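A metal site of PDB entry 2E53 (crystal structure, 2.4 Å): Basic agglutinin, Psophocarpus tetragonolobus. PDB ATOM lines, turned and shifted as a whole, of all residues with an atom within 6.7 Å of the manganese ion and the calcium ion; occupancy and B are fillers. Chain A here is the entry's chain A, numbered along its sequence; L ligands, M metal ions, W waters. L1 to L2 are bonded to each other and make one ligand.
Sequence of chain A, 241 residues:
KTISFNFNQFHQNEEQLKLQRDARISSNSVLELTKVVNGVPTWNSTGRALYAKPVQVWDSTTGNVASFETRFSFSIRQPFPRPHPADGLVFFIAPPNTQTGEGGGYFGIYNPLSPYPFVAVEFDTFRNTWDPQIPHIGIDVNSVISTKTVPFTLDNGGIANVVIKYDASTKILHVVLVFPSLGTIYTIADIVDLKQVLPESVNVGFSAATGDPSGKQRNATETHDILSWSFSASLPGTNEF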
ATOM      1  N   ASP A  87      11.931 -17.026  -5.461  1.00  0.00           N
ATOM      2  CA  ASP A  87      11.746 -18.395  -4.935  1.00  0.00           C
ATOM      3  C   ASP A  87      11.661 -18.425  -3.406  1.00  0.00           C
ATOM      4  O   ASP A  87      11.061 -19.318  -2.806  1.00  0.00           O
ATOM      5  CB  ASP A  87      12.915 -19.296  -5.365  1.00  0.00           C
ATOM      6  CG  ASP A  87      12.646 -20.026  -6.679  1.00  0.00           C
ATOM      7  OD1 ASP A  87      13.133 -19.559  -7.739  1.00  0.00           O
ATOM      8  OD2 ASP A  87      11.938 -21.061  -6.644  1.00  0.00           O
ATOM      9  N   GLY A 104      17.164 -20.697  -8.011  1.00  0.00           N
ATOM     10  CA  GLY A 104      15.805 -21.231  -7.999  1.00  0.00           C
ATOM     11  C   GLY A 104      15.397 -21.834  -6.669  1.00  0.00           C
ATOM     12  O   GLY A 104      15.685 -21.262  -5.599  1.00  0.00           O
ATOM     13  N   GLY A 105      14.744 -22.996  -6.726  1.00  0.00           N
ATOM     14  CA  GLY A 105      14.269 -23.694  -5.542  1.00  0.00           C
ATOM     15  C   GLY A 105      15.353 -24.163  -4.630  1.00  0.00           C
ATOM     16  O   GLY A 105      15.056 -24.669  -3.550  1.00  0.00           O
ATOM     17  N   TYR A 106      16.607 -24.001  -5.038  1.00  0.00           N
ATOM     18  CA  TYR A 106      17.745 -24.406  -4.192  1.00  0.00           C
ATOM     19  C   TYR A 106      18.314 -23.213  -3.391  1.00  0.00           C
ATOM     20  O   TYR A 106      19.305 -23.351  -2.671  1.00  0.00           O
ATOM     21  CB  TYR A 106      18.832 -25.039  -5.049  1.00  0.00           C
ATOM     22  CG  TYR A 106      18.412 -26.332  -5.672  1.00  0.00           C
ATOM     23  CD1 TYR A 106      18.069 -27.426  -4.874  1.00  0.00           C
ATOM     24  CD2 TYR A 106      18.351 -26.475  -7.053  1.00  0.00           C
ATOM     25  CE1 TYR A 106      17.673 -28.642  -5.451  1.00  0.00           C
ATOM     26  CE2 TYR A 106      17.947 -27.686  -7.636  1.00  0.00           C
ATOM     27  CZ  TYR A 106      17.612 -28.760  -6.831  1.00  0.00           C
ATOM     28  OH  TYR A 106      17.243 -29.948  -7.420  1.00  0.00           O
ATOM     29  N   PHE A 107      17.690 -22.054  -3.574  1.00  0.00           N
ATOM     30  CA  PHE A 107      18.022 -20.834  -2.848  1.00  0.00           C
ATOM     31  C   PHE A 107      19.463 -20.387  -2.884  1.00  0.00           C
ATOM     32  O   PHE A 107      19.823 -19.441  -2.190  1.00  0.00           O
ATOM     33  CB  PHE A 107      17.621 -20.986  -1.360  1.00  0.00           C
ATOM     34  CG  PHE A 107      16.236 -21.526  -1.149  1.00  0.00           C
ATOM     35  CD1 PHE A 107      15.124 -20.776  -1.490  1.00  0.00           C
ATOM     36  CD2 PHE A 107      16.048 -22.772  -0.564  1.00  0.00           C
ATOM     37  CE1 PHE A 107      13.815 -21.265  -1.228  1.00  0.00           C
ATOM     38  CE2 PHE A 107      14.773 -23.263  -0.309  1.00  0.00           C
ATOM     39  CZ  PHE A 107      13.646 -22.513  -0.632  1.00  0.00           C
ATOM     40  N   GLU A 122      14.027 -22.043   5.865  1.00  0.00           N
ATOM     41  CA  GLU A 122      13.558 -21.416   4.649  1.00  0.00           C
ATOM     42  C   GLU A 122      12.192 -20.759   4.767  1.00  0.00           C
ATOM     43  O   GLU A 122      11.343 -21.144   5.561  1.00  0.00           O
ATOM     44  CB  GLU A 122      13.504 -22.444   3.511  1.00  0.00           C
ATOM     45  CG  GLU A 122      12.529 -23.559   3.820  1.00  0.00           C
ATOM     46  CD  GLU A 122      12.258 -24.483   2.640  1.00  0.00           C
ATOM     47  OE1 GLU A 122      13.227 -25.055   2.075  1.00  0.00           O
ATOM     48  OE2 GLU A 122      11.076 -24.642   2.306  1.00  0.00           O
ATOM     49  N   ASP A 124       9.893 -20.248   1.967  1.00  0.00           N
ATOM     50  CA  ASP A 124       9.657 -20.684   0.608  1.00  0.00           C
ATOM     51  C   ASP A 124       8.405 -20.103  -0.003  1.00  0.00           C
ATOM     52  O   ASP A 124       7.315 -20.283   0.524  1.00  0.00           O
ATOM     53  CB  ASP A 124       9.575 -22.209   0.599  1.00  0.00           C
ATOM     54  CG  ASP A 124       9.873 -22.799  -0.751  1.00  0.00           C
ATOM     55  OD1 ASP A 124       9.633 -22.132  -1.796  1.00  0.00           O
ATOM     56  OD2 ASP A 124      10.312 -23.934  -0.761  1.00  0.00           O
ATOM     57  N   THR A 125       8.580 -19.442  -1.150  1.00  0.00           N
ATOM     58  CA  THR A 125       7.462 -18.795  -1.837  1.00  0.00           C
ATOM     59  C   THR A 125       7.005 -19.462  -3.156  1.00  0.00           C
ATOM     60  O   THR A 125       5.958 -19.088  -3.717  1.00  0.00           O
ATOM     61  CB  THR A 125       7.816 -17.319  -2.120  1.00  0.00           C
ATOM     62  OG1 THR A 125       9.057 -17.248  -2.822  1.00  0.00           O
ATOM     63  CG2 THR A 125       7.904 -16.556  -0.806  1.00  0.00           C
ATOM     64  N   PHE A 126       7.795 -20.418  -3.657  1.00  0.00           N
ATOM     65  CA  PHE A 126       7.465 -21.119  -4.894  1.00  0.00           C
ATOM     66  C   PHE A 126       7.333 -22.613  -4.648  1.00  0.00           C
ATOM     67  O   PHE A 126       8.199 -23.232  -4.020  1.00  0.00           O
ATOM     68  CB  PHE A 126       8.536 -20.904  -5.943  1.00  0.00           C
ATOM     69  CG  PHE A 126       8.229 -21.605  -7.241  1.00  0.00           C
ATOM     70  CD1 PHE A 126       7.356 -21.031  -8.171  1.00  0.00           C
ATOM     71  CD2 PHE A 126       8.811 -22.843  -7.534  1.00  0.00           C
ATOM     72  CE1 PHE A 126       7.062 -21.680  -9.378  1.00  0.00           C
ATOM     73  CE2 PHE A 126       8.524 -23.496  -8.735  1.00  0.00           C
ATOM     74  CZ  PHE A 126       7.661 -22.927  -9.645  1.00  0.00           C
ATOM     75  N   ARG A 127       6.246 -23.198  -5.137  1.00  0.00           N
ATOM     76  CA  ARG A 127       6.044 -24.620  -4.926  1.00  0.00           C
ATOM     77  C   ARG A 127       6.735 -25.519  -5.940  1.00  0.00           C
ATOM     78  O   ARG A 127       6.263 -25.685  -7.040  1.00  0.00           O
ATOM     79  CB  ARG A 127       4.548 -24.950  -4.892  1.00  0.00           C
ATOM     80  CG  ARG A 127       4.302 -26.390  -4.486  1.00  0.00           C
ATOM     81  CD  ARG A 127       2.826 -26.702  -4.289  1.00  0.00           C
ATOM     82  NE  ARG A 127       2.658 -28.055  -3.738  1.00  0.00           N
ATOM     83  CZ  ARG A 127       1.495 -28.578  -3.383  1.00  0.00           C
ATOM     84  NH1 ARG A 127       0.370 -27.884  -3.542  1.00  0.00           N
ATOM     85  NH2 ARG A 127       1.453 -29.804  -2.869  1.00  0.00           N
ATOM     86  N   ASN A 128       7.878 -26.073  -5.560  1.00  0.00           N
ATOM     87  CA  ASN A 128       8.610 -26.983  -6.423  1.00  0.00           C
ATOM     88  C   ASN A 128       7.924 -28.349  -6.319  1.00  0.00           C
ATOM     89  O   ASN A 128       6.931 -28.513  -5.602  1.00  0.00           O
ATOM     90  CB  ASN A 128      10.065 -27.097  -5.981  1.00  0.00           C
ATOM     91  CG  ASN A 128      10.929 -25.936  -6.469  1.00  0.00           C
ATOM     92  OD1 ASN A 128      11.160 -24.966  -5.742  1.00  0.00           O
ATOM     93  ND2 ASN A 128      11.426 -26.034  -7.706  1.00  0.00           N
ATOM     94  N   TRP A 130       8.938 -30.995  -4.881  1.00  0.00           N
ATOM     95  CA  TRP A 130       9.145 -31.550  -3.540  1.00  0.00           C
ATOM     96  C   TRP A 130       8.478 -30.743  -2.417  1.00  0.00           C
ATOM     97  O   TRP A 130       8.591 -31.127  -1.249  1.00  0.00           O
ATOM     98  CB  TRP A 130      10.636 -31.652  -3.270  1.00  0.00           C
ATOM     99  CG  TRP A 130      11.328 -30.330  -3.398  1.00  0.00           C
ATOM    100  CD1 TRP A 130      11.299 -29.285  -2.511  1.00  0.00           C
ATOM    101  CD2 TRP A 130      12.128 -29.874  -4.512  1.00  0.00           C
ATOM    102  NE1 TRP A 130      12.014 -28.213  -2.993  1.00  0.00           N
ATOM    103  CE2 TRP A 130      12.537 -28.553  -4.217  1.00  0.00           C
ATOM    104  CE3 TRP A 130      12.532 -30.461  -5.710  1.00  0.00           C
ATOM    105  CZ2 TRP A 130      13.338 -27.806  -5.096  1.00  0.00           C
ATOM    106  CZ3 TRP A 130      13.334 -29.726  -6.582  1.00  0.00           C
ATOM    107  CH2 TRP A 130      13.723 -28.413  -6.269  1.00  0.00           C
ATOM    108  N   ASP A 131       7.796 -29.650  -2.770  1.00  0.00           N
ATOM    109  CA  ASP A 131       7.156 -28.769  -1.795  1.00  0.00           C
ATOM    110  C   ASP A 131       5.682 -28.939  -1.547  1.00  0.00           C
ATOM    111  O   ASP A 131       4.948 -29.395  -2.413  1.00  0.00           O
ATOM    112  CB  ASP A 131       7.305 -27.282  -2.189  1.00  0.00           C
ATOM    113  CG  ASP A 131       8.683 -26.735  -1.988  1.00  0.00           C
ATOM    114  OD1 ASP A 131       9.337 -27.062  -0.975  1.00  0.00           O
ATOM    115  OD2 ASP A 131       9.118 -25.941  -2.845  1.00  0.00           O
ATOM    116  N   PRO A 132       5.232 -28.556  -0.343  1.00  0.00           N
ATOM    117  CA  PRO A 132       3.837 -28.599   0.079  1.00  0.00           C
ATOM    118  C   PRO A 132       3.339 -27.193  -0.276  1.00  0.00           C
ATOM    119  O   PRO A 132       4.081 -26.415  -0.855  1.00  0.00           O
ATOM    120  CB  PRO A 132       3.927 -28.810   1.593  1.00  0.00           C
ATOM    121  CG  PRO A 132       5.178 -28.089   1.937  1.00  0.00           C
ATOM    122  CD  PRO A 132       6.118 -28.520   0.839  1.00  0.00           C
ATOM    123  N   ILE A 134       2.524 -23.328  -0.587  1.00  0.00           N
ATOM    124  CA  ILE A 134       3.365 -22.179  -0.228  1.00  0.00           C
ATOM    125  C   ILE A 134       2.452 -20.976   0.034  1.00  0.00           C
ATOM    126  O   ILE A 134       1.296 -20.964  -0.375  1.00  0.00           O
ATOM    127  CB  ILE A 134       4.419 -21.808  -1.329  1.00  0.00           C
ATOM    128  CG1 ILE A 134       3.772 -21.685  -2.728  1.00  0.00           C
ATOM    129  CG2 ILE A 134       5.525 -22.835  -1.345  1.00  0.00           C
ATOM    130  CD1 ILE A 134       2.904 -20.421  -2.906  1.00  0.00           C
ATOM    131  N   HIS A 136       5.587 -21.241   2.920  1.00  0.00           N
ATOM    132  CA  HIS A 136       5.737 -22.047   4.124  1.00  0.00           C
ATOM    133  C   HIS A 136       7.138 -21.892   4.711  1.00  0.00           C
ATOM    134  O   HIS A 136       8.095 -21.523   4.019  1.00  0.00           O
ATOM    135  CB  HIS A 136       5.456 -23.535   3.845  1.00  0.00           C
ATOM    136  CG  HIS A 136       6.350 -24.161   2.810  1.00  0.00           C
ATOM    137  ND1 HIS A 136       5.908 -24.507   1.558  1.00  0.00           N
ATOM    138  CD2 HIS A 136       7.675 -24.480   2.857  1.00  0.00           C
ATOM    139  CE1 HIS A 136       6.924 -25.018   0.862  1.00  0.00           C
ATOM    140  NE2 HIS A 136       7.997 -25.011   1.625  1.00  0.00           N
ATOM    141  N   ILE A 137       7.228 -22.154   6.015  1.00  0.00           N
ATOM    142  CA  ILE A 137       8.499 -22.115   6.704  1.00  0.00           C
ATOM    143  C   ILE A 137       8.965 -23.557   6.691  1.00  0.00           C
ATOM    144  O   ILE A 137       8.155 -24.483   6.791  1.00  0.00           O
ATOM    145  CB  ILE A 137       8.350 -21.681   8.174  1.00  0.00           C
ATOM    146  CG1 ILE A 137       7.562 -20.378   8.277  1.00  0.00           C
ATOM    147  CG2 ILE A 137       9.714 -21.497   8.776  1.00  0.00           C
ATOM    148  CD1 ILE A 137       7.333 -19.930   9.698  1.00  0.00           C
ATOM    149  N   GLY A 138      10.265 -23.755   6.564  1.00  0.00           N
ATOM    150  CA  GLY A 138      10.773 -25.104   6.537  1.00  0.00           C
ATOM    151  C   GLY A 138      12.118 -25.210   7.202  1.00  0.00           C
ATOM    152  O   GLY A 138      12.917 -24.277   7.191  1.00  0.00           O
ATOM    153  N   ASP A 140      15.463 -27.212   6.964  1.00  0.00           N
ATOM    154  CA  ASP A 140      16.229 -28.007   6.024  1.00  0.00           C
ATOM    155  C   ASP A 140      17.561 -28.483   6.549  1.00  0.00           C
ATOM    156  O   ASP A 140      18.346 -27.710   7.057  1.00  0.00           O
ATOM    157  CB  ASP A 140      16.474 -27.204   4.728  1.00  0.00           C
ATOM    158  CG  ASP A 140      15.202 -26.659   4.113  1.00  0.00           C
ATOM    159  OD1 ASP A 140      14.111 -27.208   4.382  1.00  0.00           O
ATOM    160  OD2 ASP A 140      15.282 -25.693   3.342  1.00  0.00           O
ATOM    161  N   VAL A 144      16.888 -29.456   0.489  1.00  0.00           N
ATOM    162  CA  VAL A 144      15.828 -28.467   0.474  1.00  0.00           C
ATOM    163  C   VAL A 144      14.479 -29.154   0.618  1.00  0.00           C
ATOM    164  O   VAL A 144      13.428 -28.512   0.574  1.00  0.00           O
ATOM    165  CB  VAL A 144      16.000 -27.490  -0.761  1.00  0.00           C
ATOM    166  CG1 VAL A 144      17.454 -27.016  -0.792  1.00  0.00           C
ATOM    167  CG2 VAL A 144      15.685 -28.174  -2.072  1.00  0.00           C
ATOM    168  N   ILE A 145      14.523 -30.456   0.833  1.00  0.00           N
ATOM    169  CA  ILE A 145      13.292 -31.229   1.082  1.00  0.00           C
ATOM    170  C   ILE A 145      13.178 -31.226   2.603  1.00  0.00           C
ATOM    171  O   ILE A 145      13.706 -32.102   3.286  1.00  0.00           O
ATOM    172  CB  ILE A 145      13.412 -32.681   0.560  1.00  0.00           C
ATOM    173  CG1 ILE A 145      13.658 -32.668  -0.951  1.00  0.00           C
ATOM    174  CG2 ILE A 145      12.140 -33.421   0.832  1.00  0.00           C
ATOM    175  CD1 ILE A 145      13.892 -34.024  -1.537  1.00  0.00           C
ATOM    176  N   SER A 146      12.509 -30.184   3.111  1.00  0.00           N
ATOM    177  CA  SER A 146      12.328 -29.942   4.562  1.00  0.00           C
ATOM    178  C   SER A 146      11.921 -31.144   5.408  1.00  0.00           C
ATOM    179  O   SER A 146      11.190 -32.010   4.974  1.00  0.00           O
ATOM    180  CB  SER A 146      11.295 -28.833   4.760  1.00  0.00           C
ATOM    181  OG  SER A 146      11.622 -27.698   3.994  1.00  0.00           O
ATOM    182  N   THR A 149       7.575 -28.568   7.911  1.00  0.00           N
ATOM    183  CA  THR A 149       7.129 -27.319   7.305  1.00  0.00           C
ATOM    184  C   THR A 149       5.854 -26.846   7.972  1.00  0.00           C
ATOM    185  O   THR A 149       5.169 -27.606   8.633  1.00  0.00           O
ATOM    186  CB  THR A 149       6.831 -27.454   5.797  1.00  0.00           C
ATOM    187  OG1 THR A 149       5.786 -28.407   5.603  1.00  0.00           O
ATOM    188  CG2 THR A 149       8.080 -27.872   5.014  1.00  0.00           C
HETATM  189  C1  LIG L   1      10.869 -26.444 -15.141  1.00  0.00           C
HETATM  190  C2  LIG L   1      11.317 -25.316 -14.172  1.00  0.00           C
HETATM  191  C3  LIG L   1      10.527 -25.414 -12.838  1.00  0.00           C
HETATM  192  C4  LIG L   1       9.027 -25.373 -13.143  1.00  0.00           C
HETATM  193  C5  LIG L   1       8.665 -26.517 -14.122  1.00  0.00           C
HETATM  194  C6  LIG L   1       7.177 -26.476 -14.458  1.00  0.00           C
HETATM  195  O1  LIG L   1      11.213 -27.705 -14.630  1.00  0.00           O
HETATM  196  O2  LIG L   1      12.723 -25.431 -13.915  1.00  0.00           O
HETATM  197  O3  LIG L   1      10.852 -24.347 -11.890  1.00  0.00           O
HETATM  198  O4  LIG L   1       8.682 -24.116 -13.690  1.00  0.00           O
HETATM  199  O5  LIG L   1       9.432 -26.378 -15.364  1.00  0.00           O
HETATM  200  O6  LIG L   1       6.814 -27.522 -15.362  1.00  0.00           O
HETATM  201  C1  LG2 L   2      11.918 -23.419 -12.068  1.00  0.00           C
HETATM  202  C2  LG2 L   2      12.793 -23.400 -10.783  1.00  0.00           C
HETATM  203  C3  LG2 L   2      11.906 -22.898  -9.608  1.00  0.00           C
HETATM  204  C4  LG2 L   2      11.396 -21.492  -9.932  1.00  0.00           C
HETATM  205  C5  LG2 L   2      10.604 -21.541 -11.270  1.00  0.00           C
HETATM  206  C6  LG2 L   2      10.115 -20.147 -11.664  1.00  0.00           C
HETATM  207  O1  LG2 L   2      13.285 -24.712 -10.504  1.00  0.00           O
HETATM  208  O2  LG2 L   2      12.627 -22.887  -8.386  1.00  0.00           O
HETATM  209  O3  LG2 L   2      12.502 -20.586 -10.054  1.00  0.00           O
HETATM  210  O4  LG2 L   2      11.440 -22.080 -12.342  1.00  0.00           O
HETATM  211  O5  LG2 L   2       9.383 -20.187 -12.876  1.00  0.00           O
HETATM  212 MN    MN M   1      10.152 -25.717   0.581  1.00  0.00          MN
HETATM  213 CA    CA M   2      10.315 -23.960  -3.306  1.00  0.00          CA
HETATM  214  O   HOH W   1      10.105 -27.641   1.856  1.00  0.00           O
HETATM  215  O   HOH W   2      12.441 -25.001  -2.736  1.00  0.00           O
HETATM  216  O   HOH W   3      12.271 -26.230  -0.136  1.00  0.00           O
HETATM  217  O   HOH W   4      11.288 -22.030  -4.091  1.00  0.00           O
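The calcium ion is bound by water W4 (2.3 Å), the backbone carbonyl oxygen (O) of Phe 126 (2.3 Å), the side-chain carboxylate (OD2) of Asp 131 (2.4 Å), water W2 (2.4 Å), the side-chain carboxylate (OD1) of Asp 124 (2.5 Å), the side-chain carboxylate (OD2) of Asp 124 (2.5 Å) and the side-chain amide oxygen (OD1) of Asn 128 (2.8 Å).
Of the 23 residues printed, 4 come within 4 Å of the calcium ion.
An oxygen (O2) of LG2 L2 lies within hydrogen-bond range of the backbone NH (N) of Gly 105, at 2.7 Å. ND2 of Asn 128 sits at hydrogen-bond distance from O2 of LG2 L2, at 3.4 Å. OD1 of Asp 87 sits at hydrogen-bond distance from O3 of LG2 L2, 2.6 Å away.
Water W3 lies within hydrogen-bond range of O of Val 144 (2.7 Å), OE1 of Glu 122 (2.7 Å) and NE1 of Trp 130 (3.5 Å). Water W2 bridges O of Gly 105 (2.8 Å) and NE1 of Trp 130 (3.3 Å).
N of Glu 122 lies within hydrogen-bond range of O of Gly 138 (2.8 Å). OE1 of Glu 122 lies close to OD2 of Asp 140 (2.5 Å). The backbone carbonyl oxygen of Asp 131 lies within hydrogen-bond range of the guanidinium group of Arg 127 (3.0 Å).
Of the 23 residues printed, 4 come within 4 Å of the manganese ion. The nearest printed residue that does not touch the manganese ion is Ser 146 (4.2 Å).
The manganese ion is bound by the side-chain carboxylate of Asp 131 (2.2 Å), the side-chain carboxylate of Glu 122 (2.2 Å), the side-chain carboxylate of Asp 124 (2.2 Å), water W3 (2.3 Å), water W1 (2.3 Å) and a ring nitrogen (NE2) of His 136 (2.5 Å).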
